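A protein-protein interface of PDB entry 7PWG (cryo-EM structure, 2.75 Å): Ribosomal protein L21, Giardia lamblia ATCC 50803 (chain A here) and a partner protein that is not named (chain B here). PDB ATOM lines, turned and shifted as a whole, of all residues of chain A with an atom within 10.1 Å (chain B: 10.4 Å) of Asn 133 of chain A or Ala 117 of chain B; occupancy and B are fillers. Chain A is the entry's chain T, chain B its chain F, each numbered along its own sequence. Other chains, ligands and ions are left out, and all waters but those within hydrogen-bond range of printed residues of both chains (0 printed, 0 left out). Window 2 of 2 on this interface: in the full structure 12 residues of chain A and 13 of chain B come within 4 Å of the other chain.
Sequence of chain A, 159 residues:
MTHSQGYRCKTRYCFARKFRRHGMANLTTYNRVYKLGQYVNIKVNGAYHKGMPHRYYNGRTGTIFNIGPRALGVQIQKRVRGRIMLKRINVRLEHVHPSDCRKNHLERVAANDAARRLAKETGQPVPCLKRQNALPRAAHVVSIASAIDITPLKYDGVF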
ATOM      1  N   LEU A 129     -24.369 -19.592   8.674  1.00  0.00           N
ATOM      2  CA  LEU A 129     -23.734 -18.344   8.276  1.00  0.00           C
ATOM      3  C   LEU A 129     -22.377 -18.127   8.929  1.00  0.00           C
ATOM      4  O   LEU A 129     -21.713 -17.134   8.628  1.00  0.00           O
ATOM      5  CB  LEU A 129     -24.667 -17.168   8.580  1.00  0.00           C
ATOM      6  CG  LEU A 129     -25.896 -17.135   7.660  1.00  0.00           C
ATOM      7  CD1 LEU A 129     -26.949 -16.128   8.090  1.00  0.00           C
ATOM      8  CD2 LEU A 129     -25.474 -16.868   6.249  1.00  0.00           C
ATOM      9  N   LYS A 130     -21.942 -19.037   9.795  1.00  0.00           N
ATOM     10  CA  LYS A 130     -20.590 -18.978  10.324  1.00  0.00           C
ATOM     11  C   LYS A 130     -19.571 -19.261   9.231  1.00  0.00           C
ATOM     12  O   LYS A 130     -19.788 -20.110   8.367  1.00  0.00           O
ATOM     13  CB  LYS A 130     -20.425 -19.976  11.464  1.00  0.00           C
ATOM     14  CG  LYS A 130     -20.785 -19.417  12.807  1.00  0.00           C
ATOM     15  CD  LYS A 130     -20.178 -20.237  13.918  1.00  0.00           C
ATOM     16  CE  LYS A 130     -20.925 -21.529  14.094  1.00  0.00           C
ATOM     17  NZ  LYS A 130     -22.283 -21.293  14.656  1.00  0.00           N
ATOM     18  N   ARG A 131     -18.457 -18.530   9.264  1.00  0.00           N
ATOM     19  CA  ARG A 131     -17.325 -18.855   8.408  1.00  0.00           C
ATOM     20  C   ARG A 131     -16.768 -20.220   8.783  1.00  0.00           C
ATOM     21  O   ARG A 131     -16.789 -20.625   9.946  1.00  0.00           O
ATOM     22  CB  ARG A 131     -16.226 -17.800   8.531  1.00  0.00           C
ATOM     23  CG  ARG A 131     -16.350 -16.612   7.605  1.00  0.00           C
ATOM     24  CD  ARG A 131     -15.257 -15.590   7.884  1.00  0.00           C
ATOM     25  NE  ARG A 131     -15.347 -15.105   9.249  1.00  0.00           N
ATOM     26  CZ  ARG A 131     -14.506 -14.254   9.806  1.00  0.00           C
ATOM     27  NH1 ARG A 131     -14.684 -13.881  11.059  1.00  0.00           N
ATOM     28  NH2 ARG A 131     -13.484 -13.786   9.123  1.00  0.00           N
ATOM     29  N   GLN A 132     -16.255 -20.930   7.788  1.00  0.00           N
ATOM     30  CA  GLN A 132     -15.791 -22.300   7.967  1.00  0.00           C
ATOM     31  C   GLN A 132     -14.337 -22.396   7.531  1.00  0.00           C
ATOM     32  O   GLN A 132     -14.015 -22.106   6.376  1.00  0.00           O
ATOM     33  CB  GLN A 132     -16.664 -23.268   7.166  1.00  0.00           C
ATOM     34  CG  GLN A 132     -16.465 -24.715   7.502  1.00  0.00           C
ATOM     35  CD  GLN A 132     -16.781 -25.003   8.940  1.00  0.00           C
ATOM     36  OE1 GLN A 132     -17.625 -24.343   9.536  1.00  0.00           O
ATOM     37  NE2 GLN A 132     -16.100 -25.980   9.515  1.00  0.00           N
ATOM     38  N   ASN A 133     -13.464 -22.797   8.451  1.00  0.00           N
ATOM     39  CA  ASN A 133     -12.080 -23.060   8.084  1.00  0.00           C
ATOM     40  C   ASN A 133     -12.010 -24.381   7.335  1.00  0.00           C
ATOM     41  O   ASN A 133     -12.522 -25.390   7.815  1.00  0.00           O
ATOM     42  CB  ASN A 133     -11.187 -23.098   9.324  1.00  0.00           C
ATOM     43  CG  ASN A 133     -11.127 -21.768  10.049  1.00  0.00           C
ATOM     44  OD1 ASN A 133     -11.003 -20.719   9.439  1.00  0.00           O
ATOM     45  ND2 ASN A 133     -11.212 -21.815  11.359  1.00  0.00           N
ATOM     46  N   ALA A 134     -11.360 -24.372   6.171  1.00  0.00           N
ATOM     47  CA  ALA A 134     -11.412 -25.451   5.189  1.00  0.00           C
ATOM     48  C   ALA A 134     -11.333 -26.823   5.829  1.00  0.00           C
ATOM     49  O   ALA A 134     -10.388 -27.128   6.557  1.00  0.00           O
ATOM     50  CB  ALA A 134     -10.278 -25.291   4.176  1.00  0.00           C
ATOM     51  N   LEU A 135     -12.321 -27.645   5.551  1.00  0.00           N
ATOM     52  CA  LEU A 135     -12.493 -28.991   6.070  1.00  0.00           C
ATOM     53  C   LEU A 135     -11.735 -30.003   5.227  1.00  0.00           C
ATOM     54  O   LEU A 135     -11.335 -29.715   4.095  1.00  0.00           O
ATOM     55  CB  LEU A 135     -13.977 -29.341   6.100  1.00  0.00           C
ATOM     56  CG  LEU A 135     -14.786 -28.514   7.100  1.00  0.00           C
ATOM     57  CD1 LEU A 135     -16.190 -28.250   6.613  1.00  0.00           C
ATOM     58  CD2 LEU A 135     -14.810 -29.213   8.446  1.00  0.00           C
ATOM     59  N   PRO A 136     -11.472 -31.190   5.770  1.00  0.00           N
ATOM     60  CA  PRO A 136     -10.937 -32.273   4.938  1.00  0.00           C
ATOM     61  C   PRO A 136     -11.941 -32.716   3.883  1.00  0.00           C
ATOM     62  O   PRO A 136     -13.149 -32.730   4.116  1.00  0.00           O
ATOM     63  CB  PRO A 136     -10.652 -33.389   5.948  1.00  0.00           C
ATOM     64  CG  PRO A 136     -11.386 -32.992   7.191  1.00  0.00           C
ATOM     65  CD  PRO A 136     -11.422 -31.523   7.202  1.00  0.00           C
ATOM     66  N   ARG A 137     -11.418 -33.113   2.719  1.00  0.00           N
ATOM     67  CA  ARG A 137     -12.257 -33.454   1.574  1.00  0.00           C
ATOM     68  C   ARG A 137     -13.093 -34.699   1.849  1.00  0.00           C
ATOM     69  O   ARG A 137     -12.713 -35.566   2.633  1.00  0.00           O
ATOM     70  CB  ARG A 137     -11.407 -33.695   0.327  1.00  0.00           C
ATOM     71  CG  ARG A 137     -10.158 -32.851   0.235  1.00  0.00           C
ATOM     72  CD  ARG A 137      -9.168 -33.403  -0.789  1.00  0.00           C
ATOM     73  NE  ARG A 137      -7.920 -32.635  -0.802  1.00  0.00           N
ATOM     74  CZ  ARG A 137      -6.738 -33.103  -0.403  1.00  0.00           C
ATOM     75  NH1 ARG A 137      -6.621 -34.350   0.029  1.00  0.00           N
ATOM     76  NH2 ARG A 137      -5.667 -32.328  -0.444  1.00  0.00           N
ATOM     77  N   LYS B  77     -10.998 -36.905  10.359  1.00  0.00           N
ATOM     78  CA  LYS B  77     -11.606 -35.748  10.988  1.00  0.00           C
ATOM     79  C   LYS B  77     -11.107 -35.500  12.399  1.00  0.00           C
ATOM     80  O   LYS B  77     -11.153 -34.355  12.852  1.00  0.00           O
ATOM     81  CB  LYS B  77     -13.128 -35.892  10.989  1.00  0.00           C
ATOM     82  CG  LYS B  77     -13.618 -36.449   9.676  1.00  0.00           C
ATOM     83  CD  LYS B  77     -15.067 -36.174   9.414  1.00  0.00           C
ATOM     84  CE  LYS B  77     -15.295 -34.759   8.955  1.00  0.00           C
ATOM     85  NZ  LYS B  77     -16.714 -34.556   8.536  1.00  0.00           N
ATOM     86  N   ILE B  97       1.666 -22.598  21.344  1.00  0.00           N
ATOM     87  CA  ILE B  97       0.844 -23.533  20.584  1.00  0.00           C
ATOM     88  C   ILE B  97       0.563 -24.785  21.398  1.00  0.00           C
ATOM     89  O   ILE B  97      -0.575 -25.260  21.462  1.00  0.00           O
ATOM     90  CB  ILE B  97       1.517 -23.865  19.244  1.00  0.00           C
ATOM     91  CG1 ILE B  97       1.464 -22.667  18.317  1.00  0.00           C
ATOM     92  CG2 ILE B  97       0.860 -25.070  18.608  1.00  0.00           C
ATOM     93  CD1 ILE B  97       2.239 -22.839  17.058  1.00  0.00           C
ATOM     94  N   LEU B 100      -2.253 -24.347  24.083  1.00  0.00           N
ATOM     95  CA  LEU B 100      -3.610 -24.333  23.561  1.00  0.00           C
ATOM     96  C   LEU B 100      -4.086 -25.726  23.186  1.00  0.00           C
ATOM     97  O   LEU B 100      -5.288 -25.989  23.204  1.00  0.00           O
ATOM     98  CB  LEU B 100      -3.694 -23.406  22.360  1.00  0.00           C
ATOM     99  CG  LEU B 100      -3.307 -21.948  22.593  1.00  0.00           C
ATOM    100  CD1 LEU B 100      -3.246 -21.220  21.286  1.00  0.00           C
ATOM    101  CD2 LEU B 100      -4.270 -21.273  23.540  1.00  0.00           C
ATOM    102  N   LEU B 101      -3.169 -26.619  22.816  1.00  0.00           N
ATOM    103  CA  LEU B 101      -3.499 -28.021  22.607  1.00  0.00           C
ATOM    104  C   LEU B 101      -3.609 -28.780  23.907  1.00  0.00           C
ATOM    105  O   LEU B 101      -3.978 -29.952  23.880  1.00  0.00           O
ATOM    106  CB  LEU B 101      -2.453 -28.712  21.734  1.00  0.00           C
ATOM    107  CG  LEU B 101      -2.220 -28.248  20.305  1.00  0.00           C
ATOM    108  CD1 LEU B 101      -0.933 -28.837  19.773  1.00  0.00           C
ATOM    109  CD2 LEU B 101      -3.370 -28.635  19.450  1.00  0.00           C
ATOM    110  N   MET B 112      -8.081 -34.188  18.846  1.00  0.00           N
ATOM    111  CA  MET B 112      -7.960 -32.893  18.190  1.00  0.00           C
ATOM    112  C   MET B 112      -8.680 -32.907  16.851  1.00  0.00           C
ATOM    113  O   MET B 112      -8.529 -33.851  16.077  1.00  0.00           O
ATOM    114  CB  MET B 112      -6.489 -32.540  18.017  1.00  0.00           C
ATOM    115  CG  MET B 112      -6.208 -31.185  17.426  1.00  0.00           C
ATOM    116  SD  MET B 112      -4.964 -31.341  16.138  1.00  0.00           S
ATOM    117  CE  MET B 112      -4.262 -29.712  16.118  1.00  0.00           C
ATOM    118  N   ARG B 113      -9.442 -31.857  16.579  1.00  0.00           N
ATOM    119  CA  ARG B 113     -10.177 -31.701  15.331  1.00  0.00           C
ATOM    120  C   ARG B 113      -9.233 -31.320  14.191  1.00  0.00           C
ATOM    121  O   ARG B 113      -8.200 -30.692  14.408  1.00  0.00           O
ATOM    122  CB  ARG B 113     -11.250 -30.631  15.527  1.00  0.00           C
ATOM    123  CG  ARG B 113     -12.293 -30.533  14.469  1.00  0.00           C
ATOM    124  CD  ARG B 113     -12.958 -29.159  14.482  1.00  0.00           C
ATOM    125  NE  ARG B 113     -13.638 -28.850  15.736  1.00  0.00           N
ATOM    126  CZ  ARG B 113     -14.951 -28.911  15.921  1.00  0.00           C
ATOM    127  NH1 ARG B 113     -15.750 -29.271  14.936  1.00  0.00           N
ATOM    128  NH2 ARG B 113     -15.464 -28.605  17.097  1.00  0.00           N
ATOM    129  N   CYS B 114      -9.596 -31.688  12.963  1.00  0.00           N
ATOM    130  CA  CYS B 114      -8.772 -31.398  11.786  1.00  0.00           C
ATOM    131  C   CYS B 114      -9.461 -30.362  10.904  1.00  0.00           C
ATOM    132  O   CYS B 114     -10.530 -30.623  10.351  1.00  0.00           O
ATOM    133  CB  CYS B 114      -8.480 -32.660  10.975  1.00  0.00           C
ATOM    134  SG  CYS B 114      -7.713 -34.044  11.843  1.00  0.00           S
ATOM    135  N   ASN B 115      -8.847 -29.190  10.778  1.00  0.00           N
ATOM    136  CA  ASN B 115      -9.195 -28.201   9.764  1.00  0.00           C
ATOM    137  C   ASN B 115      -7.937 -27.401   9.488  1.00  0.00           C
ATOM    138  O   ASN B 115      -6.877 -27.684  10.038  1.00  0.00           O
ATOM    139  CB  ASN B 115     -10.377 -27.307  10.183  1.00  0.00           C
ATOM    140  CG  ASN B 115     -10.245 -26.757  11.585  1.00  0.00           C
ATOM    141  OD1 ASN B 115      -9.266 -26.984  12.266  1.00  0.00           O
ATOM    142  ND2 ASN B 115     -11.244 -26.027  12.018  1.00  0.00           N
ATOM    143  N   LYS B 116      -8.041 -26.401   8.622  1.00  0.00           N
ATOM    144  CA  LYS B 116      -6.828 -25.689   8.255  1.00  0.00           C
ATOM    145  C   LYS B 116      -6.306 -24.807   9.381  1.00  0.00           C
ATOM    146  O   LYS B 116      -5.116 -24.475   9.384  1.00  0.00           O
ATOM    147  CB  LYS B 116      -7.051 -24.868   7.001  1.00  0.00           C
ATOM    148  CG  LYS B 116      -5.744 -24.461   6.360  1.00  0.00           C
ATOM    149  CD  LYS B 116      -5.938 -23.735   5.071  1.00  0.00           C
ATOM    150  CE  LYS B 116      -4.612 -23.233   4.581  1.00  0.00           C
ATOM    151  NZ  LYS B 116      -4.487 -23.307   3.111  1.00  0.00           N
ATOM    152  N   ALA B 117      -7.156 -24.430  10.338  1.00  0.00           N
ATOM    153  CA  ALA B 117      -6.677 -23.688  11.496  1.00  0.00           C
ATOM    154  C   ALA B 117      -5.844 -24.578  12.411  1.00  0.00           C
ATOM    155  O   ALA B 117      -4.753 -24.193  12.837  1.00  0.00           O
ATOM    156  CB  ALA B 117      -7.855 -23.077  12.251  1.00  0.00           C
ATOM    157  N   THR B 118      -6.340 -25.778  12.718  1.00  0.00           N
ATOM    158  CA  THR B 118      -5.613 -26.675  13.608  1.00  0.00           C
ATOM    159  C   THR B 118      -4.443 -27.359  12.911  1.00  0.00           C
ATOM    160  O   THR B 118      -3.418 -27.611  13.543  1.00  0.00           O
ATOM    161  CB  THR B 118      -6.547 -27.732  14.201  1.00  0.00           C
ATOM    162  OG1 THR B 118      -7.274 -28.375  13.160  1.00  0.00           O
ATOM    163  CG2 THR B 118      -7.496 -27.126  15.191  1.00  0.00           C
ATOM    164  N   LEU B 119      -4.578 -27.696  11.626  1.00  0.00           N
ATOM    165  CA  LEU B 119      -3.499 -28.415  10.950  1.00  0.00           C
ATOM    166  C   LEU B 119      -2.256 -27.553  10.804  1.00  0.00           C
ATOM    167  O   LEU B 119      -1.139 -28.049  10.959  1.00  0.00           O
ATOM    168  CB  LEU B 119      -3.949 -28.924   9.584  1.00  0.00           C
ATOM    169  CG  LEU B 119      -4.959 -30.085   9.573  1.00  0.00           C
ATOM    170  CD1 LEU B 119      -5.391 -30.434   8.162  1.00  0.00           C
ATOM    171  CD2 LEU B 119      -4.438 -31.299  10.306  1.00  0.00           C
ATOM    172  N   ASN B 120      -2.425 -26.269  10.507  1.00  0.00           N
ATOM    173  CA  ASN B 120      -1.276 -25.415  10.246  1.00  0.00           C
ATOM    174  C   ASN B 120      -0.557 -25.021  11.515  1.00  0.00           C
ATOM    175  O   ASN B 120       0.638 -24.718  11.469  1.00  0.00           O
ATOM    176  CB  ASN B 120      -1.698 -24.164   9.494  1.00  0.00           C
ATOM    177  CG  ASN B 120      -1.856 -24.406   8.028  1.00  0.00           C
ATOM    178  OD1 ASN B 120      -1.922 -25.544   7.578  1.00  0.00           O
ATOM    179  ND2 ASN B 120      -1.928 -23.331   7.266  1.00  0.00           N
ATOM    180  N   ALA B 121      -1.255 -24.990  12.645  1.00  0.00           N
ATOM    181  CA  ALA B 121      -0.563 -24.762  13.901  1.00  0.00           C
ATOM    182  C   ALA B 121       0.238 -25.984  14.313  1.00  0.00           C
ATOM    183  O   ALA B 121       1.330 -25.854  14.868  1.00  0.00           O
ATOM    184  CB  ALA B 121      -1.552 -24.378  14.994  1.00  0.00           C
ATOM    185  N   LEU B 122      -0.294 -27.173  14.044  1.00  0.00           N
ATOM    186  CA  LEU B 122       0.321 -28.410  14.507  1.00  0.00           C
ATOM    187  C   LEU B 122       1.581 -28.739  13.726  1.00  0.00           C
ATOM    188  O   LEU B 122       2.506 -29.335  14.277  1.00  0.00           O
ATOM    189  CB  LEU B 122      -0.692 -29.540  14.404  1.00  0.00           C
ATOM    190  CG  LEU B 122      -0.193 -30.968  14.549  1.00  0.00           C
ATOM    191  CD1 LEU B 122      -0.008 -31.322  16.004  1.00  0.00           C
ATOM    192  CD2 LEU B 122      -1.174 -31.876  13.867  1.00  0.00           C
ATOM    193  N   ARG B 123       1.648 -28.343  12.461  1.00  0.00           N
ATOM    194  CA  ARG B 123       2.873 -28.512  11.692  1.00  0.00           C
ATOM    195  C   ARG B 123       4.013 -27.629  12.193  1.00  0.00           C
ATOM    196  O   ARG B 123       5.169 -27.941  11.922  1.00  0.00           O
ATOM    197  CB  ARG B 123       2.588 -28.260  10.213  1.00  0.00           C
ATOM    198  CG  ARG B 123       3.773 -28.481   9.275  1.00  0.00           C
ATOM    199  CD  ARG B 123       3.369 -28.418   7.803  1.00  0.00           C
ATOM    200  NE  ARG B 123       2.837 -27.115   7.421  1.00  0.00           N
ATOM    201  CZ  ARG B 123       1.843 -26.939   6.555  1.00  0.00           C
ATOM    202  NH1 ARG B 123       1.265 -27.987   5.986  1.00  0.00           N
ATOM    203  NH2 ARG B 123       1.425 -25.716   6.264  1.00  0.00           N
ATOM    204  N   ILE B 124       3.733 -26.574  12.958  1.00  0.00           N
ATOM    205  CA  ILE B 124       4.800 -25.766  13.553  1.00  0.00           C
ATOM    206  C   ILE B 124       5.509 -26.498  14.697  1.00  0.00           C
ATOM    207  O   ILE B 124       6.703 -26.288  14.931  1.00  0.00           O
ATOM    208  CB  ILE B 124       4.238 -24.413  14.016  1.00  0.00           C
ATOM    209  CG1 ILE B 124       3.996 -23.499  12.823  1.00  0.00           C
ATOM    210  CG2 ILE B 124       5.154 -23.731  15.011  1.00  0.00           C
ATOM    211  CD1 ILE B 124       3.417 -22.217  13.209  1.00  0.00           C
ATOM    212  N   VAL B 125       4.813 -27.372  15.408  1.00  0.00           N
ATOM    213  CA  VAL B 125       5.379 -28.015  16.583  1.00  0.00           C
ATOM    214  C   VAL B 125       5.591 -29.502  16.326  1.00  0.00           C
ATOM    215  O   VAL B 125       5.555 -30.311  17.253  1.00  0.00           O
ATOM    216  CB  VAL B 125       4.488 -27.767  17.816  1.00  0.00           C
ATOM    217  CG1 VAL B 125       4.398 -26.279  18.089  1.00  0.00           C
ATOM    218  CG2 VAL B 125       3.104 -28.328  17.614  1.00  0.00           C
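N of Lys 116 of chain B is in hydrogen-bond range of O of Ala 134 of chain A (3.2 Å).
The backbone carbonyl oxygen of Lys 77 of chain B is in hydrogen-bond range of the backbone NH of Cys 114 of chain B (3.1 Å).
The side-chain hydroxyl of Thr 118 of chain B is in hydrogen-bond range of the side-chain amide oxygen of Asn 115 of chain B.
Among the printed residues, pairs that only touch across the chains: Pro 136 of chain A with Cys 114 of chain B (3.4 Å), Ala 134 of chain A with Asn 115 of chain B (3.6 Å), Asn 133 of chain A with Ala 117 of chain B (3.7 Å) and Asn 133 of chain A with Asn 115 of chain B (3.7 Å).
Leu 129 of chain A touches none of the printed residues of chain B.
No residue of chain B comes within 4 Å of Gln 132 of chain A.
Of chain B, only Asn 115 (3.6 Å) and Lys 116 (3.2 Å) come within 4 Å of Ala 134 of chain A.
No residue of chain B comes within 4 Å of Leu 135 of chain A.
Printed residues of chain B within 4 Å of Pro 136 of chain A: Cys 114.
Printed residues of chain A within 4 Å of Cys 114 of chain B: Pro 136 (3.4 Å).
Of the printed residues of chain A, Asn 115 of chain B touches Asn 133 (3.7 Å) and Ala 134 (3.6 Å).
Of the printed residues of chain A, Lys 116 of chain B touches Ala 134 (3.2 Å).
Of the printed residues of chain A, Ala 117 of chain B touches Asn 133 (3.7 Å).
Leu 122 of chain B touches none of the printed residues of chain A.
The nearest residue of chain B that does not touch Asn 133 of chain A is Lys 116 of chain B (4.6 Å).
The nearest printed residue of chain A that does not touch Lys 116 of chain B is Asn 133 of chain A (4.6 Å).
Hydrophobic or aromatic side chains of chain B within 4 Å of the printed part of chain A: Ala 117.
Of the 9 printed residues of chain A, 3 touch a printed residue of chain B.
Hydrophobic or aromatic side chains of chain A within 4 Å of the printed part of chain B: Pro 136.
Among the printed residues, 5 pairs touch across the chains.
Among the printed residues, no Asp or Glu carboxylate lies within 4 Å of a Lys or Arg side-chain nitrogen of the other chain.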
